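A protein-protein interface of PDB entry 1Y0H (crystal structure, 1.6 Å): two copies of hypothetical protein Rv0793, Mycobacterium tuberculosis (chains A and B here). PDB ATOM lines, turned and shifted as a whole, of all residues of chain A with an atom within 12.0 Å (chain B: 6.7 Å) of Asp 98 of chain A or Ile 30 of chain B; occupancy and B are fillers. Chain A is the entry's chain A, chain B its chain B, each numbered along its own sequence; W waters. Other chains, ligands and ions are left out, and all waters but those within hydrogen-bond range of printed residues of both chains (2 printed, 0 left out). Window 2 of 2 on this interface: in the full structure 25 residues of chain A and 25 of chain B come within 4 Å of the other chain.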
ATOM      1  N   SER A   4      24.349   3.764 -17.165  1.00  0.00           N
ATOM      2  CA  SER A   4      23.442   4.489 -16.269  1.00  0.00           C
ATOM      3  C   SER A   4      23.525   5.989 -16.510  1.00  0.00           C
ATOM      4  O   SER A   4      24.614   6.511 -16.727  1.00  0.00           O
ATOM      5  CB  SER A   4      23.804   4.216 -14.806  1.00  0.00           C
ATOM      6  OG  SER A   4      23.821   2.821 -14.555  1.00  0.00           O
ATOM      7  N   PRO A   5      22.380   6.695 -16.424  1.00  0.00           N
ATOM      8  CA  PRO A   5      22.429   8.153 -16.555  1.00  0.00           C
ATOM      9  C   PRO A   5      23.310   8.827 -15.511  1.00  0.00           C
ATOM     10  O   PRO A   5      23.497   8.314 -14.397  1.00  0.00           O
ATOM     11  CB  PRO A   5      20.970   8.591 -16.361  1.00  0.00           C
ATOM     12  CG  PRO A   5      20.162   7.379 -16.601  1.00  0.00           C
ATOM     13  CD  PRO A   5      21.004   6.201 -16.227  1.00  0.00           C
ATOM     14  N   VAL A   6      23.850   9.976 -15.898  1.00  0.00           N
ATOM     15  CA  VAL A   6      24.710  10.751 -15.027  1.00  0.00           C
ATOM     16  C   VAL A   6      24.370  12.211 -15.198  1.00  0.00           C
ATOM     17  O   VAL A   6      23.753  12.596 -16.197  1.00  0.00           O
ATOM     18  CB  VAL A   6      26.246  10.528 -15.320  1.00  0.00           C
ATOM     19  CG1 VAL A   6      26.654   9.095 -15.071  1.00  0.00           C
ATOM     20  CG2 VAL A   6      26.652  10.995 -16.742  1.00  0.00           C
ATOM     21  N   ALA A   7      24.764  13.012 -14.213  1.00  0.00           N
ATOM     22  CA  ALA A   7      24.693  14.465 -14.331  1.00  0.00           C
ATOM     23  C   ALA A   7      26.059  15.086 -14.019  1.00  0.00           C
ATOM     24  O   ALA A   7      26.929  14.450 -13.448  1.00  0.00           O
ATOM     25  CB  ALA A   7      23.595  15.046 -13.419  1.00  0.00           C
ATOM     26  N   ARG A  40      20.624  14.589 -22.277  1.00  0.00           N
ATOM     27  CA  ARG A  40      19.253  14.818 -21.832  1.00  0.00           C
ATOM     28  C   ARG A  40      18.975  16.310 -21.601  1.00  0.00           C
ATOM     29  O   ARG A  40      17.936  16.822 -22.009  1.00  0.00           O
ATOM     30  CB  ARG A  40      18.936  14.015 -20.575  1.00  0.00           C
ATOM     31  CG  ARG A  40      17.667  14.482 -19.904  1.00  0.00           C
ATOM     32  CD  ARG A  40      17.329  13.646 -18.714  1.00  0.00           C
ATOM     33  NE  ARG A  40      16.279  14.282 -17.923  1.00  0.00           N
ATOM     34  CZ  ARG A  40      15.674  13.702 -16.892  1.00  0.00           C
ATOM     35  NH1 ARG A  40      16.000  12.462 -16.537  1.00  0.00           N
ATOM     36  NH2 ARG A  40      14.726  14.351 -16.230  1.00  0.00           N
ATOM     37  N   PHE A  56      24.394  22.979 -15.463  1.00  0.00           N
ATOM     38  CA  PHE A  56      23.891  21.688 -15.026  1.00  0.00           C
ATOM     39  C   PHE A  56      23.640  20.850 -16.271  1.00  0.00           C
ATOM     40  O   PHE A  56      22.910  21.263 -17.162  1.00  0.00           O
ATOM     41  CB  PHE A  56      22.620  21.820 -14.183  1.00  0.00           C
ATOM     42  CG  PHE A  56      22.271  20.556 -13.461  1.00  0.00           C
ATOM     43  CD1 PHE A  56      21.263  19.725 -13.924  1.00  0.00           C
ATOM     44  CD2 PHE A  56      22.974  20.185 -12.332  1.00  0.00           C
ATOM     45  CE1 PHE A  56      20.954  18.533 -13.255  1.00  0.00           C
ATOM     46  CE2 PHE A  56      22.676  18.992 -11.654  1.00  0.00           C
ATOM     47  CZ  PHE A  56      21.666  18.167 -12.133  1.00  0.00           C
ATOM     48  N   ARG A  58      22.907  16.843 -17.961  1.00  0.00           N
ATOM     49  CA  ARG A  58      22.413  15.487 -17.748  1.00  0.00           C
ATOM     50  C   ARG A  58      22.628  14.676 -19.014  1.00  0.00           C
ATOM     51  O   ARG A  58      22.258  15.119 -20.097  1.00  0.00           O
ATOM     52  CB  ARG A  58      20.912  15.515 -17.446  1.00  0.00           C
ATOM     53  CG  ARG A  58      20.499  16.062 -16.096  1.00  0.00           C
ATOM     54  CD  ARG A  58      18.966  15.976 -16.049  1.00  0.00           C
ATOM     55  NE  ARG A  58      18.366  16.460 -14.811  1.00  0.00           N
ATOM     56  CZ  ARG A  58      17.836  17.668 -14.656  1.00  0.00           C
ATOM     57  NH1 ARG A  58      17.310  18.008 -13.489  1.00  0.00           N
ATOM     58  NH2 ARG A  58      17.844  18.540 -15.659  1.00  0.00           N
ATOM     59  N   LEU A  94      27.848  13.413 -11.063  1.00  0.00           N
ATOM     60  CA  LEU A  94      26.776  12.987 -10.168  1.00  0.00           C
ATOM     61  C   LEU A  94      26.058  11.729 -10.640  1.00  0.00           C
ATOM     62  O   LEU A  94      25.747  11.586 -11.825  1.00  0.00           O
ATOM     63  CB  LEU A  94      25.752  14.108  -9.999  1.00  0.00           C
ATOM     64  CG  LEU A  94      26.242  15.474  -9.497  1.00  0.00           C
ATOM     65  CD1 LEU A  94      25.120  16.496  -9.660  1.00  0.00           C
ATOM     66  CD2 LEU A  94      26.677  15.386  -8.043  1.00  0.00           C
ATOM     67  N   ALA A  95      25.789  10.837  -9.692  1.00  0.00           N
ATOM     68  CA  ALA A  95      24.978   9.643  -9.945  1.00  0.00           C
ATOM     69  C   ALA A  95      23.590   9.847  -9.347  1.00  0.00           C
ATOM     70  O   ALA A  95      23.476  10.119  -8.153  1.00  0.00           O
ATOM     71  CB  ALA A  95      25.646   8.410  -9.339  1.00  0.00           C
ATOM     72  N   PRO A  96      22.531   9.743 -10.176  1.00  0.00           N
ATOM     73  CA  PRO A  96      21.173   9.932  -9.668  1.00  0.00           C
ATOM     74  C   PRO A  96      20.839   8.938  -8.574  1.00  0.00           C
ATOM     75  O   PRO A  96      21.220   7.770  -8.663  1.00  0.00           O
ATOM     76  CB  PRO A  96      20.287   9.688 -10.893  1.00  0.00           C
ATOM     77  CG  PRO A  96      21.162   9.888 -12.067  1.00  0.00           C
ATOM     78  CD  PRO A  96      22.548   9.483 -11.627  1.00  0.00           C
ATOM     79  N   LEU A  97      20.184   9.426  -7.527  1.00  0.00           N
ATOM     80  CA  LEU A  97      19.604   8.572  -6.502  1.00  0.00           C
ATOM     81  C   LEU A  97      18.079   8.604  -6.658  1.00  0.00           C
ATOM     82  O   LEU A  97      17.411   7.565  -6.595  1.00  0.00           O
ATOM     83  CB  LEU A  97      20.031   9.026  -5.100  1.00  0.00           C
ATOM     84  CG  LEU A  97      21.511   8.952  -4.705  1.00  0.00           C
ATOM     85  CD1 LEU A  97      21.672   9.347  -3.249  1.00  0.00           C
ATOM     86  CD2 LEU A  97      22.120   7.570  -4.937  1.00  0.00           C
ATOM     87  N   ASP A  98      17.537   9.797  -6.879  1.00  0.00           N
ATOM     88  CA  ASP A  98      16.132   9.972  -7.234  1.00  0.00           C
ATOM     89  C   ASP A  98      15.982  11.186  -8.137  1.00  0.00           C
ATOM     90  O   ASP A  98      15.861  12.326  -7.668  1.00  0.00           O
ATOM     91  CB  ASP A  98      15.236  10.106  -5.993  1.00  0.00           C
ATOM     92  CG  ASP A  98      13.741  10.105  -6.340  1.00  0.00           C
ATOM     93  OD1 ASP A  98      13.375  10.467  -7.482  1.00  0.00           O
ATOM     94  OD2 ASP A  98      12.921   9.737  -5.471  1.00  0.00           O
ATOM     95  N   GLU A  99      15.995  10.925  -9.438  1.00  0.00           N
ATOM     96  CA  GLU A  99      15.870  11.961 -10.446  1.00  0.00           C
ATOM     97  C   GLU A  99      14.613  11.679 -11.263  1.00  0.00           C
ATOM     98  O   GLU A  99      14.542  10.666 -11.959  1.00  0.00           O
ATOM     99  CB  GLU A  99      17.117  11.965 -11.331  1.00  0.00           C
ATOM    100  CG  GLU A  99      17.151  13.022 -12.421  1.00  0.00           C
ATOM    101  CD  GLU A  99      18.425  12.952 -13.236  1.00  0.00           C
ATOM    102  OE1 GLU A  99      18.855  11.824 -13.574  1.00  0.00           O
ATOM    103  OE2 GLU A  99      19.005  14.019 -13.531  1.00  0.00           O
ATOM    104  N   ALA A 100      13.625  12.569 -11.166  1.00  0.00           N
ATOM    105  CA  ALA A 100      12.355  12.410 -11.887  1.00  0.00           C
ATOM    106  C   ALA A 100      12.522  12.610 -13.391  1.00  0.00           C
ATOM    107  O   ALA A 100      13.419  13.332 -13.840  1.00  0.00           O
ATOM    108  CB  ALA A 100      11.304  13.369 -11.344  1.00  0.00           C
ATOM    109  N   SER A 101      11.650  11.968 -14.161  1.00  0.00           N
ATOM    110  CA  SER A 101      11.646  12.120 -15.607  1.00  0.00           C
ATOM    111  C   SER A 101      10.951  13.419 -16.007  1.00  0.00           C
ATOM    112  O   SER A 101      11.309  14.042 -17.013  1.00  0.00           O
ATOM    113  CB  SER A 101      10.966  10.923 -16.271  1.00  0.00           C
ATOM    114  OG  SER A 101       9.650  10.738 -15.771  1.00  0.00           O
ATOM    115  N   ARG B  23      20.597  10.291   4.246  1.00  0.00           N
ATOM    116  CA  ARG B  23      19.859   9.781   3.088  1.00  0.00           C
ATOM    117  C   ARG B  23      18.366   9.709   3.398  1.00  0.00           C
ATOM    118  O   ARG B  23      17.542  10.129   2.580  1.00  0.00           O
ATOM    119  CB  ARG B  23      20.391   8.405   2.663  1.00  0.00           C
ATOM    120  CG  ARG B  23      19.638   7.755   1.497  1.00  0.00           C
ATOM    121  CD  ARG B  23      19.716   8.569   0.202  1.00  0.00           C
ATOM    122  NE  ARG B  23      18.786   8.057  -0.809  1.00  0.00           N
ATOM    123  CZ  ARG B  23      19.050   7.039  -1.630  1.00  0.00           C
ATOM    124  NH1 ARG B  23      20.217   6.409  -1.570  1.00  0.00           N
ATOM    125  NH2 ARG B  23      18.137   6.645  -2.506  1.00  0.00           N
ATOM    126  N   LEU B  25      16.669  11.430   5.696  1.00  0.00           N
ATOM    127  CA  LEU B  25      16.145  12.784   5.860  1.00  0.00           C
ATOM    128  C   LEU B  25      15.831  13.418   4.508  1.00  0.00           C
ATOM    129  O   LEU B  25      14.778  14.039   4.320  1.00  0.00           O
ATOM    130  CB  LEU B  25      17.155  13.645   6.630  1.00  0.00           C
ATOM    131  CG  LEU B  25      16.605  14.933   7.234  1.00  0.00           C
ATOM    132  CD1 LEU B  25      15.712  14.614   8.421  1.00  0.00           C
ATOM    133  CD2 LEU B  25      17.741  15.837   7.663  1.00  0.00           C
ATOM    134  N   LEU B  26      16.742  13.240   3.554  1.00  0.00           N
ATOM    135  CA  LEU B  26      16.564  13.830   2.241  1.00  0.00           C
ATOM    136  C   LEU B  26      15.506  13.081   1.453  1.00  0.00           C
ATOM    137  O   LEU B  26      14.694  13.707   0.757  1.00  0.00           O
ATOM    138  CB  LEU B  26      17.896  13.877   1.483  1.00  0.00           C
ATOM    139  CG  LEU B  26      18.971  14.733   2.158  1.00  0.00           C
ATOM    140  CD1 LEU B  26      20.165  14.812   1.250  1.00  0.00           C
ATOM    141  CD2 LEU B  26      18.475  16.139   2.523  1.00  0.00           C
ATOM    142  N   ASP B  27      15.493  11.752   1.588  1.00  0.00           N
ATOM    143  CA  ASP B  27      14.471  10.914   0.935  1.00  0.00           C
ATOM    144  C   ASP B  27      13.064  11.413   1.265  1.00  0.00           C
ATOM    145  O   ASP B  27      12.201  11.457   0.391  1.00  0.00           O
ATOM    146  CB  ASP B  27      14.564   9.452   1.381  1.00  0.00           C
ATOM    147  CG  ASP B  27      15.603   8.643   0.607  1.00  0.00           C
ATOM    148  OD1 ASP B  27      16.182   9.144  -0.382  1.00  0.00           O
ATOM    149  OD2 ASP B  27      15.836   7.479   1.012  1.00  0.00           O
ATOM    150  N   ALA B  28      12.834  11.758   2.530  1.00  0.00           N
ATOM    151  CA  ALA B  28      11.500  12.175   2.986  1.00  0.00           C
ATOM    152  C   ALA B  28      11.061  13.546   2.443  1.00  0.00           C
ATOM    153  O   ALA B  28       9.881  13.892   2.501  1.00  0.00           O
ATOM    154  CB  ALA B  28      11.437  12.151   4.504  1.00  0.00           C
ATOM    155  N   MET B  29      12.008  14.312   1.898  1.00  0.00           N
ATOM    156  CA  MET B  29      11.702  15.622   1.339  1.00  0.00           C
ATOM    157  C   MET B  29      11.133  15.541  -0.071  1.00  0.00           C
ATOM    158  O   MET B  29      10.439  16.454  -0.520  1.00  0.00           O
ATOM    159  CB  MET B  29      12.967  16.491   1.321  1.00  0.00           C
ATOM    160  CG  MET B  29      13.358  17.016   2.695  1.00  0.00           C
ATOM    161  SD  MET B  29      12.179  18.247   3.319  1.00  0.00           S
ATOM    162  CE  MET B  29      12.492  19.583   2.163  1.00  0.00           C
ATOM    163  N   ILE B  30      11.452  14.456  -0.773  1.00  0.00           N
ATOM    164  CA  ILE B  30      11.221  14.397  -2.214  1.00  0.00           C
ATOM    165  C   ILE B  30       9.733  14.501  -2.584  1.00  0.00           C
ATOM    166  O   ILE B  30       9.341  15.395  -3.343  1.00  0.00           O
ATOM    167  CB  ILE B  30      11.916  13.172  -2.859  1.00  0.00           C
ATOM    168  CG1 ILE B  30      13.441  13.290  -2.663  1.00  0.00           C
ATOM    169  CG2 ILE B  30      11.533  13.077  -4.339  1.00  0.00           C
ATOM    170  CD1 ILE B  30      14.272  12.087  -3.105  1.00  0.00           C
ATOM    171  N   THR B  31       8.909  13.619  -2.027  1.00  0.00           N
ATOM    172  CA  THR B  31       7.464  13.607  -2.318  1.00  0.00           C
ATOM    173  C   THR B  31       6.743  14.935  -2.045  1.00  0.00           C
ATOM    174  O   THR B  31       6.145  15.501  -2.967  1.00  0.00           O
ATOM    175  CB  THR B  31       6.763  12.425  -1.617  1.00  0.00           C
ATOM    176  OG1 THR B  31       7.282  11.201  -2.152  1.00  0.00           O
ATOM    177  CG2 THR B  31       5.248  12.462  -1.826  1.00  0.00           C
ATOM    178  N   PRO B  32       6.821  15.450  -0.794  1.00  0.00           N
ATOM    179  CA  PRO B  32       6.099  16.690  -0.528  1.00  0.00           C
ATOM    180  C   PRO B  32       6.650  17.872  -1.306  1.00  0.00           C
ATOM    181  O   PRO B  32       5.891  18.764  -1.681  1.00  0.00           O
ATOM    182  CB  PRO B  32       6.275  16.896   0.986  1.00  0.00           C
ATOM    183  CG  PRO B  32       7.470  16.085   1.357  1.00  0.00           C
ATOM    184  CD  PRO B  32       7.505  14.932   0.404  1.00  0.00           C
ATOM    185  N   THR B  33       7.960  17.893  -1.550  1.00  0.00           N
ATOM    186  CA  THR B  33       8.518  19.028  -2.268  1.00  0.00           C
ATOM    187  C   THR B  33       8.057  19.017  -3.716  1.00  0.00           C
ATOM    188  O   THR B  33       7.684  20.053  -4.251  1.00  0.00           O
ATOM    189  CB  THR B  33      10.043  19.080  -2.218  1.00  0.00           C
ATOM    190  OG1 THR B  33      10.472  19.051  -0.848  1.00  0.00           O
ATOM    191  CG2 THR B  33      10.535  20.362  -2.897  1.00  0.00           C
ATOM    192  N   ARG B  34       8.082  17.846  -4.344  1.00  0.00           N
ATOM    193  CA  ARG B  34       7.664  17.752  -5.745  1.00  0.00           C
ATOM    194  C   ARG B  34       6.189  18.103  -5.895  1.00  0.00           C
ATOM    195  O   ARG B  34       5.752  18.505  -6.969  1.00  0.00           O
ATOM    196  CB  ARG B  34       7.942  16.362  -6.313  1.00  0.00           C
ATOM    197  CG  ARG B  34       9.407  16.145  -6.652  1.00  0.00           C
ATOM    198  CD  ARG B  34       9.627  14.760  -7.220  1.00  0.00           C
ATOM    199  NE  ARG B  34      11.050  14.507  -7.400  1.00  0.00           N
ATOM    200  CZ  ARG B  34      11.596  13.304  -7.572  1.00  0.00           C
ATOM    201  NH1 ARG B  34      10.842  12.215  -7.607  1.00  0.00           N
ATOM    202  NH2 ARG B  34      12.911  13.199  -7.714  1.00  0.00           N
ATOM    203  N   ALA B  35       5.447  17.972  -4.800  1.00  0.00           N
ATOM    204  CA  ALA B  35       4.005  18.242  -4.763  1.00  0.00           C
ATOM    205  C   ALA B  35       3.655  19.732  -4.568  1.00  0.00           C
ATOM    206  O   ALA B  35       2.481  20.123  -4.690  1.00  0.00           O
ATOM    207  CB  ALA B  35       3.346  17.386  -3.682  1.00  0.00           C
ATOM    208  N   TYR B  42      12.944  18.514  -8.416  1.00  0.00           N
ATOM    209  CA  TYR B  42      13.662  18.295  -7.152  1.00  0.00           C
ATOM    210  C   TYR B  42      14.320  16.927  -7.215  1.00  0.00           C
ATOM    211  O   TYR B  42      13.675  15.896  -6.990  1.00  0.00           O
ATOM    212  CB  TYR B  42      12.669  18.356  -5.997  1.00  0.00           C
ATOM    213  CG  TYR B  42      13.229  18.435  -4.594  1.00  0.00           C
ATOM    214  CD1 TYR B  42      13.606  19.660  -4.042  1.00  0.00           C
ATOM    215  CD2 TYR B  42      13.305  17.294  -3.790  1.00  0.00           C
ATOM    216  CE1 TYR B  42      14.073  19.740  -2.736  1.00  0.00           C
ATOM    217  CE2 TYR B  42      13.767  17.361  -2.469  1.00  0.00           C
ATOM    218  CZ  TYR B  42      14.163  18.589  -1.961  1.00  0.00           C
ATOM    219  OH  TYR B  42      14.608  18.700  -0.666  1.00  0.00           O
ATOM    220  N   ASP B  43      15.611  16.910  -7.525  1.00  0.00           N
ATOM    221  CA  ASP B  43      16.291  15.654  -7.822  1.00  0.00           C
ATOM    222  C   ASP B  43      17.487  15.429  -6.908  1.00  0.00           C
ATOM    223  O   ASP B  43      18.187  16.383  -6.562  1.00  0.00           O
ATOM    224  CB  ASP B  43      16.740  15.669  -9.285  1.00  0.00           C
ATOM    225  CG  ASP B  43      15.568  15.749 -10.249  1.00  0.00           C
ATOM    226  OD1 ASP B  43      14.588  15.003 -10.031  1.00  0.00           O
ATOM    227  OD2 ASP B  43      15.609  16.574 -11.198  1.00  0.00           O
ATOM    228  N   LEU B  44      17.708  14.173  -6.526  1.00  0.00           N
ATOM    229  CA  LEU B  44      18.752  13.822  -5.556  1.00  0.00           C
ATOM    230  C   LEU B  44      19.857  12.971  -6.186  1.00  0.00           C
ATOM    231  O   LEU B  44      19.572  11.990  -6.881  1.00  0.00           O
ATOM    232  CB  LEU B  44      18.146  13.095  -4.345  1.00  0.00           C
ATOM    233  CG  LEU B  44      19.082  12.558  -3.255  1.00  0.00           C
ATOM    234  CD1 LEU B  44      19.777  13.692  -2.487  1.00  0.00           C
ATOM    235  CD2 LEU B  44      18.291  11.649  -2.287  1.00  0.00           C
ATOM    236  N   TYR B  45      21.115  13.345  -5.916  1.00  0.00           N
ATOM    237  CA  TYR B  45      22.288  12.671  -6.479  1.00  0.00           C
ATOM    238  C   TYR B  45      23.360  12.373  -5.436  1.00  0.00           C
ATOM    239  O   TYR B  45      23.372  12.967  -4.367  1.00  0.00           O
ATOM    240  CB  TYR B  45      22.955  13.542  -7.556  1.00  0.00           C
ATOM    241  CG  TYR B  45      22.027  14.065  -8.615  1.00  0.00           C
ATOM    242  CD1 TYR B  45      21.293  15.215  -8.391  1.00  0.00           C
ATOM    243  CD2 TYR B  45      21.916  13.434  -9.859  1.00  0.00           C
ATOM    244  CE1 TYR B  45      20.440  15.722  -9.352  1.00  0.00           C
ATOM    245  CE2 TYR B  45      21.056  13.942 -10.846  1.00  0.00           C
ATOM    246  CZ  TYR B  45      20.320  15.087 -10.569  1.00  0.00           C
ATOM    247  OH  TYR B  45      19.457  15.638 -11.498  1.00  0.00           O
ATOM    248  N   LEU B  55      21.339  17.900  -3.982  1.00  0.00           N
ATOM    249  CA  LEU B  55      19.982  18.145  -4.481  1.00  0.00           C
ATOM    250  C   LEU B  55      20.041  19.253  -5.511  1.00  0.00           C
ATOM    251  O   LEU B  55      20.682  20.288  -5.299  1.00  0.00           O
ATOM    252  CB  LEU B  55      19.032  18.574  -3.362  1.00  0.00           C
ATOM    253  CG  LEU B  55      18.461  17.526  -2.407  1.00  0.00           C
ATOM    254  CD1 LEU B  55      17.949  18.281  -1.178  1.00  0.00           C
ATOM    255  CD2 LEU B  55      17.356  16.663  -3.029  1.00  0.00           C
ATOM    256  N   HIS B  73       7.419  20.229   5.781  1.00  0.00           N
ATOM    257  CA  HIS B  73       8.471  19.245   5.518  1.00  0.00           C
ATOM    258  C   HIS B  73       9.865  19.858   5.588  1.00  0.00           C
ATOM    259  O   HIS B  73      10.764  19.281   6.183  1.00  0.00           O
ATOM    260  CB  HIS B  73       8.226  18.485   4.205  1.00  0.00           C
ATOM    261  CG  HIS B  73       7.903  19.354   3.027  1.00  0.00           C
ATOM    262  ND1 HIS B  73       6.668  19.934   2.845  1.00  0.00           N
ATOM    263  CD2 HIS B  73       8.630  19.665   1.926  1.00  0.00           C
ATOM    264  CE1 HIS B  73       6.663  20.605   1.706  1.00  0.00           C
ATOM    265  NE2 HIS B  73       7.842  20.459   1.130  1.00  0.00           N
HETATM  266  O   HOH W   1      13.920  15.963 -13.081  1.00  0.00           O
HETATM  267  O   HOH W   2      15.991  19.098 -10.633  1.00  0.00           O
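CB of Ala 7 of chain A touches CE2 of Tyr 45 of chain B, at 3.8 Å.
NE of Arg 58 of chain A touches OH of Tyr 45 of chain B, at 3.6 Å.
O of Ala 95 of chain A touches CA of Tyr 45 of chain B, at 3.3 Å.
Pro 96 of chain A touches Leu 44 of chain B.
Pro 96 of chain A touches Tyr 45 of chain B (CA to CD2, 3.6 Å).
Tyr 45 of chain B touches Leu 97 of chain A.
Ile 30 of chain B touches Asp 98 of chain A (CD1 to OD2, 3.6 Å).
Asp 98 of chain A touches Asp 43 of chain B (O to CA, 3.4 Å).
Glu 99 of chain A touches Asp 43 of chain B.
Arg 34 of chain B touches Ala 100 of chain A (NH2 to N, 3.6 Å).
Water W1 bridges OD2 of Asp 43 of chain B (2.6 Å) and O of Ala 100 of chain A (2.8 Å).
Water W2 bridges OD2 of Asp 43 of chain B (2.6 Å) and NH1 of Arg 58 of chain A (3.3 Å).
The side-chain hydroxyl of Tyr 45 of chain B sits at hydrogen-bond distance from the side-chain carboxylate of Glu 99 of chain A (2.6 Å).
O of Asp 98 of chain A sits at hydrogen-bond distance from N of Leu 44 of chain B (2.9 Å).
The backbone NH (N) of Ala 100 of chain A is in hydrogen-bond range of the side-chain carboxylate (OD1) of Asp 43 of chain B, 2.9 Å away.
The guanidinium group (NH2) of Arg 34 of chain B lies within salt-bridge range of the side-chain carboxylate (OD1) of Asp 98 of chain A (2.8 Å).
The backbone NH (N) of Leu 97 of chain A lies within hydrogen-bond range of the backbone carbonyl oxygen (O) of Leu 44 of chain B (2.7 Å).
OD2 of Asp 43 of chain B is in salt-bridge range of NH1 of Arg 58 of chain A.
Hydrophobic or aromatic side chains of chain A within 4 Å of the printed part of chain B: Ala 7, Phe 56, Leu 94, Leu 97 and Ala 100.
Along chain A the printed residues that touch a printed residue of chain B span positions 7 to 100.
Hydrophobic or aromatic side chains of chain B that line the printed part of chain A: Ile 30 and Tyr 45.
Among the printed residues, Asp or Glu carboxylates within 4 Å of a Lys or Arg side-chain nitrogen of the other chain: Arg 58 of chain A with Asp 43 of chain B (3.2 Å) and Asp 98 of chain A with Arg 34 of chain B (2.8 Å).
No position is printed for both chains.
The backbone NH (N) of Arg 40 of chain A sits at hydrogen-bond distance from the backbone carbonyl oxygen (O) of Arg 58 of chain A, at 2.8 Å.
The backbone NH of Leu 94 of chain A sits at hydrogen-bond distance from the backbone carbonyl oxygen of Ala 7 of chain A.
The guanidinium group (NH2) of Arg 34 of chain B lies within hydrogen-bond range of the backbone carbonyl oxygen (O) of Tyr 42 of chain B.
OE2 of Glu 99 of chain A is in salt-bridge range of NE of Arg 58 of chain A (2.8 Å).
The side-chain carboxylate of Asp 27 of chain B lies within salt-bridge range of the guanidinium group of Arg 23 of chain B.
The side-chain carboxylate (OD1) of Asp 43 of chain B lies within salt-bridge range of the guanidinium group (NH2) of Arg 34 of chain B (3.4 Å).
Of the printed residues of chain B, Asp 98 of chain A touches Ile 30, Arg 34, Asp 43 and Leu 44.
Ile 30 of chain B touches just one residue of chain A: Asp 98.
No residue of chain A comes within 4 Å of Leu 26 of chain B.
Met 29 of chain B touches none of the printed residues of chain A.
No residue of chain A comes within 4 Å of Pro 32 of chain B.
No residue of chain A comes within 4 Å of Thr 33 of chain B.
Arg 34 of chain B touches just these residues of chain A: Asp 98 (2.8 Å) and Ala 100 (3.6 Å).
No residue of chain A comes within 4 Å of Tyr 42 of chain B.
Leu 44 of chain B touches just these residues of chain A: Pro 96 (3.7 Å), Leu 97 (2.7 Å) and Asp 98 (2.9 Å).
Printed residues of chain A within 4 Å of Tyr 45 of chain B: Ala 7, Phe 56, Arg 58, Leu 94, Ala 95, Pro 96, Leu 97 and Glu 99.
Of the printed residues of chain B, Leu 94 of chain A touches Tyr 45 (3.8 Å).
Of the printed residues of chain B, Phe 56 of chain A touches Tyr 45 (3.4 Å).
Printed residues of chain B within 4 Å of Pro 96 of chain A: Leu 44 and Tyr 45.
Ser 4 of chain A touches none of the printed residues of chain B.
His 73 of chain B touches none of the printed residues of chain A.
The nearest residue of chain A that does not touch Ile 30 of chain B is Leu 97 of chain A (6.3 Å).
The nearest printed residue of chain B that does not touch Glu 99 of chain A is Arg 34 of chain B (4.2 Å).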
